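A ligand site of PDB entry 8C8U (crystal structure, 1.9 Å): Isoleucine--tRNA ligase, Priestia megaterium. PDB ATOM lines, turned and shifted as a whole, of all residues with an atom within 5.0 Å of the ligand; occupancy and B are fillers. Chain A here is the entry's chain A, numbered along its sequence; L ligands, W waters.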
ATOM      1  N   GLY A  45      30.878  -5.161  -5.891  1.00  0.00           N
ATOM      2  CA  GLY A  45      30.329  -4.337  -4.827  1.00  0.00           C
ATOM      3  C   GLY A  45      29.318  -5.173  -4.068  1.00  0.00           C
ATOM      4  O   GLY A  45      28.361  -5.667  -4.652  1.00  0.00           O
ATOM      5  N   PRO A  46      29.514  -5.350  -2.766  1.00  0.00           N
ATOM      6  CA  PRO A  46      28.716  -6.349  -2.042  1.00  0.00           C
ATOM      7  C   PRO A  46      27.259  -5.920  -1.928  1.00  0.00           C
ATOM      8  O   PRO A  46      26.953  -4.824  -1.425  1.00  0.00           O
ATOM      9  CB  PRO A  46      29.385  -6.436  -0.675  1.00  0.00           C
ATOM     10  CG  PRO A  46      30.078  -5.090  -0.504  1.00  0.00           C
ATOM     11  CD  PRO A  46      30.553  -4.752  -1.906  1.00  0.00           C
ATOM     12  N   PRO A  47      26.333  -6.773  -2.398  1.00  0.00           N
ATOM     13  CA  PRO A  47      24.909  -6.488  -2.305  1.00  0.00           C
ATOM     14  C   PRO A  47      24.332  -6.881  -0.949  1.00  0.00           C
ATOM     15  O   PRO A  47      25.099  -7.266  -0.075  1.00  0.00           O
ATOM     16  CB  PRO A  47      24.311  -7.364  -3.430  1.00  0.00           C
ATOM     17  CG  PRO A  47      25.174  -8.569  -3.395  1.00  0.00           C
ATOM     18  CD  PRO A  47      26.593  -8.053  -3.077  1.00  0.00           C
ATOM     19  N   HIS A  54      17.644  -7.716  -8.410  1.00  0.00           N
ATOM     20  CA  HIS A  54      16.894  -7.082  -9.487  1.00  0.00           C
ATOM     21  C   HIS A  54      17.771  -7.027 -10.742  1.00  0.00           C
ATOM     22  O   HIS A  54      18.925  -7.459 -10.722  1.00  0.00           O
ATOM     23  CB  HIS A  54      16.395  -5.684  -9.089  1.00  0.00           C
ATOM     24  CG  HIS A  54      17.469  -4.765  -8.644  1.00  0.00           C
ATOM     25  ND1 HIS A  54      18.487  -4.339  -9.480  1.00  0.00           N
ATOM     26  CD2 HIS A  54      17.673  -4.132  -7.456  1.00  0.00           C
ATOM     27  CE1 HIS A  54      19.286  -3.528  -8.806  1.00  0.00           C
ATOM     28  NE2 HIS A  54      18.814  -3.374  -7.580  1.00  0.00           N
ATOM     29  N   VAL A  55      17.206  -6.487 -11.822  1.00  0.00           N
ATOM     30  CA  VAL A  55      17.874  -6.518 -13.117  1.00  0.00           C
ATOM     31  C   VAL A  55      19.118  -5.619 -13.151  1.00  0.00           C
ATOM     32  O   VAL A  55      19.986  -5.789 -14.007  1.00  0.00           O
ATOM     33  CB  VAL A  55      16.874  -6.154 -14.244  1.00  0.00           C
ATOM     34  CG1 VAL A  55      16.508  -4.679 -14.202  1.00  0.00           C
ATOM     35  CG2 VAL A  55      17.433  -6.518 -15.634  1.00  0.00           C
ATOM     36  N   GLY A  56      19.256  -4.694 -12.206  1.00  0.00           N
ATOM     37  CA  GLY A  56      20.526  -4.004 -12.043  1.00  0.00           C
ATOM     38  C   GLY A  56      21.647  -4.952 -11.634  1.00  0.00           C
ATOM     39  O   GLY A  56      22.762  -4.869 -12.136  1.00  0.00           O
ATOM     40  N   HIS A  57      21.365  -5.841 -10.661  1.00  0.00           N
ATOM     41  CA  HIS A  57      22.343  -6.875 -10.295  1.00  0.00           C
ATOM     42  C   HIS A  57      22.611  -7.791 -11.470  1.00  0.00           C
ATOM     43  O   HIS A  57      23.751  -8.218 -11.686  1.00  0.00           O
ATOM     44  CB  HIS A  57      21.849  -7.729  -9.110  1.00  0.00           C
ATOM     45  CG  HIS A  57      21.512  -6.936  -7.878  1.00  0.00           C
ATOM     46  ND1 HIS A  57      20.213  -6.735  -7.460  1.00  0.00           N
ATOM     47  CD2 HIS A  57      22.305  -6.345  -6.952  1.00  0.00           C
ATOM     48  CE1 HIS A  57      20.225  -6.023  -6.338  1.00  0.00           C
ATOM     49  NE2 HIS A  57      21.480  -5.770  -6.018  1.00  0.00           N
ATOM     50  N   LEU A  59      22.516  -7.138 -14.669  1.00  0.00           N
ATOM     51  CA  LEU A  59      23.409  -6.474 -15.627  1.00  0.00           C
ATOM     52  C   LEU A  59      24.852  -6.499 -15.149  1.00  0.00           C
ATOM     53  O   LEU A  59      25.766  -6.898 -15.896  1.00  0.00           O
ATOM     54  CB  LEU A  59      22.926  -5.031 -15.851  1.00  0.00           C
ATOM     55  CG  LEU A  59      23.789  -4.090 -16.717  1.00  0.00           C
ATOM     56  CD1 LEU A  59      23.902  -4.620 -18.140  1.00  0.00           C
ATOM     57  CD2 LEU A  59      23.233  -2.647 -16.677  1.00  0.00           C
ATOM     58  N   ASP A  85      26.813  -7.001   2.328  1.00  0.00           N
ATOM     59  CA  ASP A  85      26.956  -5.700   2.987  1.00  0.00           C
ATOM     60  C   ASP A  85      25.768  -5.581   3.936  1.00  0.00           C
ATOM     61  O   ASP A  85      24.642  -5.309   3.506  1.00  0.00           O
ATOM     62  CB  ASP A  85      26.958  -4.589   1.922  1.00  0.00           C
ATOM     63  CG  ASP A  85      27.352  -3.195   2.460  1.00  0.00           C
ATOM     64  OD1 ASP A  85      28.016  -3.087   3.510  1.00  0.00           O
ATOM     65  OD2 ASP A  85      26.965  -2.195   1.797  1.00  0.00           O
ATOM     66  N   TRP A 517      29.290   3.080   3.939  1.00  0.00           N
ATOM     67  CA  TRP A 517      30.200   3.152   2.802  1.00  0.00           C
ATOM     68  C   TRP A 517      31.653   2.856   3.211  1.00  0.00           C
ATOM     69  O   TRP A 517      32.430   2.392   2.366  1.00  0.00           O
ATOM     70  CB  TRP A 517      30.096   4.530   2.098  1.00  0.00           C
ATOM     71  CG  TRP A 517      28.775   4.729   1.482  1.00  0.00           C
ATOM     72  CD1 TRP A 517      27.742   5.490   1.953  1.00  0.00           C
ATOM     73  CD2 TRP A 517      28.276   4.087   0.291  1.00  0.00           C
ATOM     74  NE1 TRP A 517      26.651   5.377   1.126  1.00  0.00           N
ATOM     75  CE2 TRP A 517      26.956   4.533   0.094  1.00  0.00           C
ATOM     76  CE3 TRP A 517      28.841   3.183  -0.631  1.00  0.00           C
ATOM     77  CZ2 TRP A 517      26.175   4.106  -0.994  1.00  0.00           C
ATOM     78  CZ3 TRP A 517      28.057   2.770  -1.716  1.00  0.00           C
ATOM     79  CH2 TRP A 517      26.746   3.239  -1.878  1.00  0.00           C
ATOM     80  N   SER A 520      31.967  -1.145   3.083  1.00  0.00           N
ATOM     81  CA  SER A 520      32.088  -1.704   1.730  1.00  0.00           C
ATOM     82  C   SER A 520      33.342  -1.212   1.014  1.00  0.00           C
ATOM     83  O   SER A 520      33.963  -1.968   0.242  1.00  0.00           O
ATOM     84  CB  SER A 520      30.831  -1.401   0.874  1.00  0.00           C
ATOM     85  OG  SER A 520      30.574  -0.008   0.754  1.00  0.00           O
ATOM     86  N   ALA A 548      32.863  -3.353 -12.012  1.00  0.00           N
ATOM     87  CA  ALA A 548      31.747  -3.048 -12.914  1.00  0.00           C
ATOM     88  C   ALA A 548      30.494  -2.846 -12.061  1.00  0.00           C
ATOM     89  O   ALA A 548      29.917  -3.808 -11.562  1.00  0.00           O
ATOM     90  CB  ALA A 548      31.561  -4.176 -13.921  1.00  0.00           C
ATOM     91  N   GLU A 549      30.102  -1.576 -11.854  1.00  0.00           N
ATOM     92  CA  GLU A 549      28.910  -1.251 -11.064  1.00  0.00           C
ATOM     93  C   GLU A 549      28.247  -0.035 -11.694  1.00  0.00           C
ATOM     94  O   GLU A 549      28.770   0.550 -12.639  1.00  0.00           O
ATOM     95  CB  GLU A 549      29.225  -0.985  -9.588  1.00  0.00           C
ATOM     96  CG  GLU A 549      30.050  -2.069  -8.844  1.00  0.00           C
ATOM     97  CD  GLU A 549      29.314  -3.402  -8.646  1.00  0.00           C
ATOM     98  OE1 GLU A 549      28.054  -3.423  -8.587  1.00  0.00           O
ATOM     99  OE2 GLU A 549      30.017  -4.448  -8.545  1.00  0.00           O
ATOM    100  N   GLY A 550      27.082   0.353 -11.161  1.00  0.00           N
ATOM    101  CA  GLY A 550      26.362   1.483 -11.719  1.00  0.00           C
ATOM    102  C   GLY A 550      27.134   2.778 -11.580  1.00  0.00           C
ATOM    103  O   GLY A 550      27.963   2.948 -10.686  1.00  0.00           O
ATOM    104  N   ASP A 552      25.874   5.259 -10.546  1.00  0.00           N
ATOM    105  CA  ASP A 552      25.503   5.883  -9.284  1.00  0.00           C
ATOM    106  C   ASP A 552      26.518   5.589  -8.193  1.00  0.00           C
ATOM    107  O   ASP A 552      26.419   6.175  -7.106  1.00  0.00           O
ATOM    108  CB  ASP A 552      24.091   5.440  -8.867  1.00  0.00           C
ATOM    109  CG  ASP A 552      23.988   3.937  -8.586  1.00  0.00           C
ATOM    110  OD1 ASP A 552      24.940   3.160  -8.862  1.00  0.00           O
ATOM    111  OD2 ASP A 552      22.942   3.528  -8.050  1.00  0.00           O
ATOM    112  N   GLN A 553      27.498   4.714  -8.438  1.00  0.00           N
ATOM    113  CA  GLN A 553      28.549   4.515  -7.442  1.00  0.00           C
ATOM    114  C   GLN A 553      29.678   5.564  -7.528  1.00  0.00           C
ATOM    115  O   GLN A 553      30.650   5.424  -6.801  1.00  0.00           O
ATOM    116  CB  GLN A 553      29.095   3.095  -7.565  1.00  0.00           C
ATOM    117  CG  GLN A 553      27.996   2.035  -7.372  1.00  0.00           C
ATOM    118  CD  GLN A 553      27.307   2.176  -6.023  1.00  0.00           C
ATOM    119  OE1 GLN A 553      27.961   2.460  -5.044  1.00  0.00           O
ATOM    120  NE2 GLN A 553      25.983   2.011  -5.976  1.00  0.00           N
ATOM    121  N   TRP A 557      30.349   3.530  -3.968  1.00  0.00           N
ATOM    122  CA  TRP A 557      31.408   2.536  -3.768  1.00  0.00           C
ATOM    123  C   TRP A 557      32.670   2.904  -4.553  1.00  0.00           C
ATOM    124  O   TRP A 557      33.794   2.666  -4.074  1.00  0.00           O
ATOM    125  CB  TRP A 557      30.901   1.146  -4.167  1.00  0.00           C
ATOM    126  CG  TRP A 557      31.785  -0.038  -3.746  1.00  0.00           C
ATOM    127  CD1 TRP A 557      32.217  -0.333  -2.461  1.00  0.00           C
ATOM    128  CD2 TRP A 557      32.304  -1.065  -4.591  1.00  0.00           C
ATOM    129  NE1 TRP A 557      32.956  -1.499  -2.481  1.00  0.00           N
ATOM    130  CE2 TRP A 557      33.038  -1.962  -3.771  1.00  0.00           C
ATOM    131  CE3 TRP A 557      32.223  -1.333  -5.974  1.00  0.00           C
ATOM    132  CZ2 TRP A 557      33.702  -3.077  -4.287  1.00  0.00           C
ATOM    133  CZ3 TRP A 557      32.878  -2.457  -6.492  1.00  0.00           C
ATOM    134  CH2 TRP A 557      33.605  -3.309  -5.651  1.00  0.00           C
ATOM    135  N   LEU A 580      27.818   1.368 -15.248  1.00  0.00           N
ATOM    136  CA  LEU A 580      26.579   0.782 -15.753  1.00  0.00           C
ATOM    137  C   LEU A 580      25.440   1.800 -15.666  1.00  0.00           C
ATOM    138  O   LEU A 580      25.307   2.495 -14.667  1.00  0.00           O
ATOM    139  CB  LEU A 580      26.170  -0.465 -14.945  1.00  0.00           C
ATOM    140  CG  LEU A 580      27.309  -1.466 -14.779  1.00  0.00           C
ATOM    141  CD1 LEU A 580      26.830  -2.655 -13.967  1.00  0.00           C
ATOM    142  CD2 LEU A 580      27.768  -1.928 -16.154  1.00  0.00           C
ATOM    143  N   GLY A 581      24.579   1.814 -16.684  1.00  0.00           N
ATOM    144  CA  GLY A 581      23.414   2.673 -16.671  1.00  0.00           C
ATOM    145  C   GLY A 581      22.225   1.964 -16.045  1.00  0.00           C
ATOM    146  O   GLY A 581      21.977   0.797 -16.310  1.00  0.00           O
ATOM    147  N   HIS A 582      21.480   2.699 -15.230  1.00  0.00           N
ATOM    148  CA  HIS A 582      20.274   2.160 -14.589  1.00  0.00           C
ATOM    149  C   HIS A 582      19.230   1.767 -15.639  1.00  0.00           C
ATOM    150  O   HIS A 582      18.906   2.539 -16.547  1.00  0.00           O
ATOM    151  CB  HIS A 582      19.729   3.227 -13.616  1.00  0.00           C
ATOM    152  CG  HIS A 582      18.532   2.806 -12.799  1.00  0.00           C
ATOM    153  ND1 HIS A 582      18.532   2.815 -11.421  1.00  0.00           N
ATOM    154  CD2 HIS A 582      17.272   2.453 -13.173  1.00  0.00           C
ATOM    155  CE1 HIS A 582      17.344   2.435 -10.979  1.00  0.00           C
ATOM    156  NE2 HIS A 582      16.558   2.211 -12.020  1.00  0.00           N
ATOM    157  N   VAL A 583      18.679   0.547 -15.514  1.00  0.00           N
ATOM    158  CA  VAL A 583      17.816   0.005 -16.561  1.00  0.00           C
ATOM    159  C   VAL A 583      16.490   0.769 -16.601  1.00  0.00           C
ATOM    160  O   VAL A 583      15.925   1.131 -15.568  1.00  0.00           O
ATOM    161  CB  VAL A 583      17.582  -1.504 -16.341  1.00  0.00           C
ATOM    162  CG1 VAL A 583      16.843  -2.104 -17.539  1.00  0.00           C
ATOM    163  CG2 VAL A 583      18.919  -2.234 -16.109  1.00  0.00           C
ATOM    164  N   MET A 591      13.487   2.044 -14.025  1.00  0.00           N
ATOM    165  CA  MET A 591      12.768   1.029 -13.254  1.00  0.00           C
ATOM    166  C   MET A 591      12.871   1.335 -11.790  1.00  0.00           C
ATOM    167  O   MET A 591      13.965   1.577 -11.271  1.00  0.00           O
ATOM    168  CB  MET A 591      13.345  -0.347 -13.544  1.00  0.00           C
ATOM    169  CG  MET A 591      12.972  -0.861 -14.925  1.00  0.00           C
ATOM    170  SD  MET A 591      13.611  -2.497 -15.219  1.00  0.00           S
ATOM    171  CE  MET A 591      12.906  -2.820 -16.832  1.00  0.00           C
ATOM    172  N   SER A 592      11.734   1.299 -11.088  1.00  0.00           N
ATOM    173  CA  SER A 592      11.802   1.592  -9.658  1.00  0.00           C
ATOM    174  C   SER A 592      10.754   0.801  -8.903  1.00  0.00           C
ATOM    175  O   SER A 592       9.758   0.343  -9.456  1.00  0.00           O
ATOM    176  CB  SER A 592      11.624   3.087  -9.371  1.00  0.00           C
ATOM    177  OG  SER A 592      10.255   3.450  -9.506  1.00  0.00           O
ATOM    178  N   LYS A 593      11.006   0.636  -7.607  1.00  0.00           N
ATOM    179  CA  LYS A 593      10.051  -0.067  -6.762  1.00  0.00           C
ATOM    180  C   LYS A 593       8.708   0.663  -6.733  1.00  0.00           C
ATOM    181  O   LYS A 593       7.646   0.035  -6.884  1.00  0.00           O
ATOM    182  CB  LYS A 593      10.619  -0.215  -5.348  1.00  0.00           C
ATOM    183  CG  LYS A 593       9.636  -0.841  -4.344  1.00  0.00           C
ATOM    184  CD  LYS A 593      10.150  -0.711  -2.903  1.00  0.00           C
ATOM    185  CE  LYS A 593       9.204  -1.401  -1.912  1.00  0.00           C
ATOM    186  NZ  LYS A 593       9.947  -1.937  -0.717  1.00  0.00           N
ATOM    187  N   ALA A 598       9.543  -2.448 -12.868  1.00  0.00           N
ATOM    188  CA  ALA A 598      10.710  -3.314 -12.977  1.00  0.00           C
ATOM    189  C   ALA A 598      10.329  -4.661 -13.580  1.00  0.00           C
ATOM    190  O   ALA A 598       9.230  -5.174 -13.356  1.00  0.00           O
ATOM    191  CB  ALA A 598      11.370  -3.558 -11.611  1.00  0.00           C
HETATM  192  C1  LIG L   1      19.243  -0.817 -11.873  1.00  0.00           C
HETATM  193  C2  LIG L   1      20.277  -0.388 -10.827  1.00  0.00           C
HETATM  194  C3  LIG L   1      21.743  -0.108 -11.131  1.00  0.00           C
HETATM  195  C4  LIG L   1      22.630   0.291  -9.950  1.00  0.00           C
HETATM  196  C5  LIG L   1      23.358  -0.944  -9.447  1.00  0.00           C
HETATM  197  C6  LIG L   1      24.404  -0.549  -8.366  1.00  0.00           C
HETATM  198  C7  LIG L   1      25.249  -1.765  -8.103  1.00  0.00           C
HETATM  199  C8  LIG L   1      24.355  -2.929  -7.653  1.00  0.00           C
HETATM  200  C9  LIG L   1      23.788  -2.680  -6.249  1.00  0.00           C
HETATM  201  C10 LIG L   1      24.894  -2.877  -5.179  1.00  0.00           C
HETATM  202  C11 LIG L   1      25.495  -1.629  -4.589  1.00  0.00           C
HETATM  203  C12 LIG L   1      26.926  -1.718  -4.032  1.00  0.00           C
HETATM  204  C13 LIG L   1      27.133  -0.646  -2.955  1.00  0.00           C
HETATM  205  C14 LIG L   1      28.369  -1.011  -2.102  1.00  0.00           C
HETATM  206  C15 LIG L   1      22.321  -0.284 -12.518  1.00  0.00           C
HETATM  207  C16 LIG L   1      23.223  -3.143  -8.695  1.00  0.00           C
HETATM  208  C17 LIG L   1      10.041  -4.289  -7.389  1.00  0.00           C
HETATM  209  O1  LIG L   1       9.548  -4.543  -8.520  1.00  0.00           O
HETATM  210  O2  LIG L   1       9.506  -3.600  -6.498  1.00  0.00           O
HETATM  211  C18 LIG L   1      11.391  -4.907  -7.018  1.00  0.00           C
HETATM  212  C19 LIG L   1      12.558  -4.352  -7.835  1.00  0.00           C
HETATM  213  C20 LIG L   1      12.516  -2.830  -7.969  1.00  0.00           C
HETATM  214  C21 LIG L   1      13.944  -2.289  -8.250  1.00  0.00           C
HETATM  215  C22 LIG L   1      14.134  -2.056  -9.742  1.00  0.00           C
HETATM  216  C23 LIG L   1      15.535  -1.496 -10.133  1.00  0.00           C
HETATM  217  C24 LIG L   1      15.991  -2.223 -11.386  1.00  0.00           C
HETATM  218  C25 LIG L   1      17.013  -1.393 -12.175  1.00  0.00           C
HETATM  219  O3  LIG L   1      18.056  -1.054 -11.280  1.00  0.00           O
HETATM  220  O4  LIG L   1      19.423  -0.929 -13.090  1.00  0.00           O
HETATM  221  O5  LIG L   1      22.464  -1.940  -8.922  1.00  0.00           O
HETATM  222  O6  LIG L   1      25.926  -2.084  -9.322  1.00  0.00           O
HETATM  223  O7  LIG L   1      25.252   0.487  -8.884  1.00  0.00           O
HETATM  224  O8  LIG L   1      24.510  -2.385  -3.865  1.00  0.00           O
HETATM  225  C26 LIG L   1      27.938  -1.522  -5.171  1.00  0.00           C
HETATM  226  O9  LIG L   1      25.994  -0.592  -2.096  1.00  0.00           O
HETATM  227  O   HOH W   1      24.264   1.551  -3.517  1.00  0.00           O
HETATM  228  O   HOH W   2       7.207  -2.632  -6.663  1.00  0.00           O
HETATM  229  O   HOH W   3      25.587  -2.728  -0.552  1.00  0.00           O
HETATM  230  O   HOH W   4      26.949  -5.114  -6.768  1.00  0.00           O
HETATM  231  O   HOH W   5       8.921  -2.364  -9.950  1.00  0.00           O
HETATM  232  O   HOH W   6      14.552  -5.950  -5.469  1.00  0.00           O
HETATM  233  O   HOH W   7      20.615  -0.826  -7.046  1.00  0.00           O
HETATM  234  O   HOH W   8      14.365  -3.333  -4.951  1.00  0.00           O
HETATM  235  O   HOH W   9      25.299  -4.108 -11.060  1.00  0.00           O
HETATM  236  O   HOH W  10      10.177  -6.629  -9.850  1.00  0.00           O
HETATM  237  O   HOH W  11      21.860  -2.101  -2.946  1.00  0.00           O
HETATM  238  O   HOH W  12      10.636  -4.016  -3.770  1.00  0.00           O
HETATM  239  O   HOH W  13      25.718   1.181   0.364  1.00  0.00           O
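Residues that only touch the ligand: Gly 56 (3.4 Å), Lys 593 (3.5 Å), His 582 (3.5 Å), His 54 (3.6 Å), Met 591 (3.6 Å), Ala 598 (3.7 Å), Gly 45 (3.7 Å), Ser 520 (3.7 Å), Trp 517 (3.7 Å), His 57 (3.8 Å), Val 55 (3.8 Å), Trp 557 (3.9 Å) and Gly 581 (3.96 Å). Hydrophobic or aromatic side chains within 4 Å of the ligand: His 54, Val 55, His 57, Trp 517, Trp 557, His 582, Val 583, Met 591 and Ala 598. Within 4 Å of the ligand: Gly 45, His 54, Val 55, Gly 56, His 57, Trp 517, Ser 520, Glu 549, Gly 550, Asp 552, Gln 553, Trp 557, Gly 581, His 582, Val 583, Met 591, Lys 593 and Ala 598. Along chain A the residues within 4 Å of the ligand span positions 45 to 598.
The side-chain amide oxygen (OE1) of Gln 553 lies within hydrogen-bond range of the backbone NH (N) of Trp 557, 2.8 Å away. The backbone NH of Gly 56 lies within hydrogen-bond range of a ring nitrogen (ND1) of His 54 (2.9 Å). N of Leu 580 is in hydrogen-bond range of O of Glu 549. The backbone NH (N) of Met 591 is in hydrogen-bond range of the backbone carbonyl oxygen (O) of Val 583 (3.0 Å). N of His 54 sits at hydrogen-bond distance from ND1 of His 57. NE2 of Gln 553 sits at hydrogen-bond distance from OD1 of Asp 552 (3.3 Å). The indole nitrogen (NE1) of Trp 557 lies within hydrogen-bond range of the backbone carbonyl oxygen (O) of Ser 520. The backbone carbonyl oxygen (O) of Trp 517 sits at hydrogen-bond distance from the side-chain hydroxyl (OG) of Ser 520 (3.4 Å).
The backbone NH (N) of Gly 550 lies within hydrogen-bond range of an oxygen (O7) of the ligand, 2.9 Å away. O4 of the ligand sits at hydrogen-bond distance from N of Val 583 (2.9 Å). OD1 of Asp 552 lies within hydrogen-bond range of O7 of the ligand. An oxygen (O6) of the ligand sits at hydrogen-bond distance from the side-chain carboxylate of Glu 549, 2.6 Å away. An oxygen (O7) of the ligand sits at hydrogen-bond distance from the side-chain amide nitrogen (NE2) of Gln 553.
Water W2 lies within hydrogen-bond range of an oxygen (O2) of the ligand and the backbone carbonyl oxygen of Lys 593. Water W3 lies within hydrogen-bond range of O of Pro 46 (2.6 Å), O9 of the ligand (2.7 Å) and OD2 of Asp 85 (2.8 Å). Water W5 lies within hydrogen-bond range of O1 of the ligand (2.7 Å), O of Ser 592 (2.9 Å) and N of Ala 598 (3.0 Å). Water W9 bridges O6 of the ligand (2.7 Å) and O of Gly 56 (2.9 Å). Water W1 lies within hydrogen-bond range of the side-chain amide nitrogen (NE2) of Gln 553 (3.0 Å) and an oxygen (O9) of the ligand (3.1 Å). Water W4 lies within hydrogen-bond range of the backbone carbonyl oxygen (O) of Gly 45 (2.6 Å) and the side-chain carboxylate (OE1) of Glu 549 (2.7 Å).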
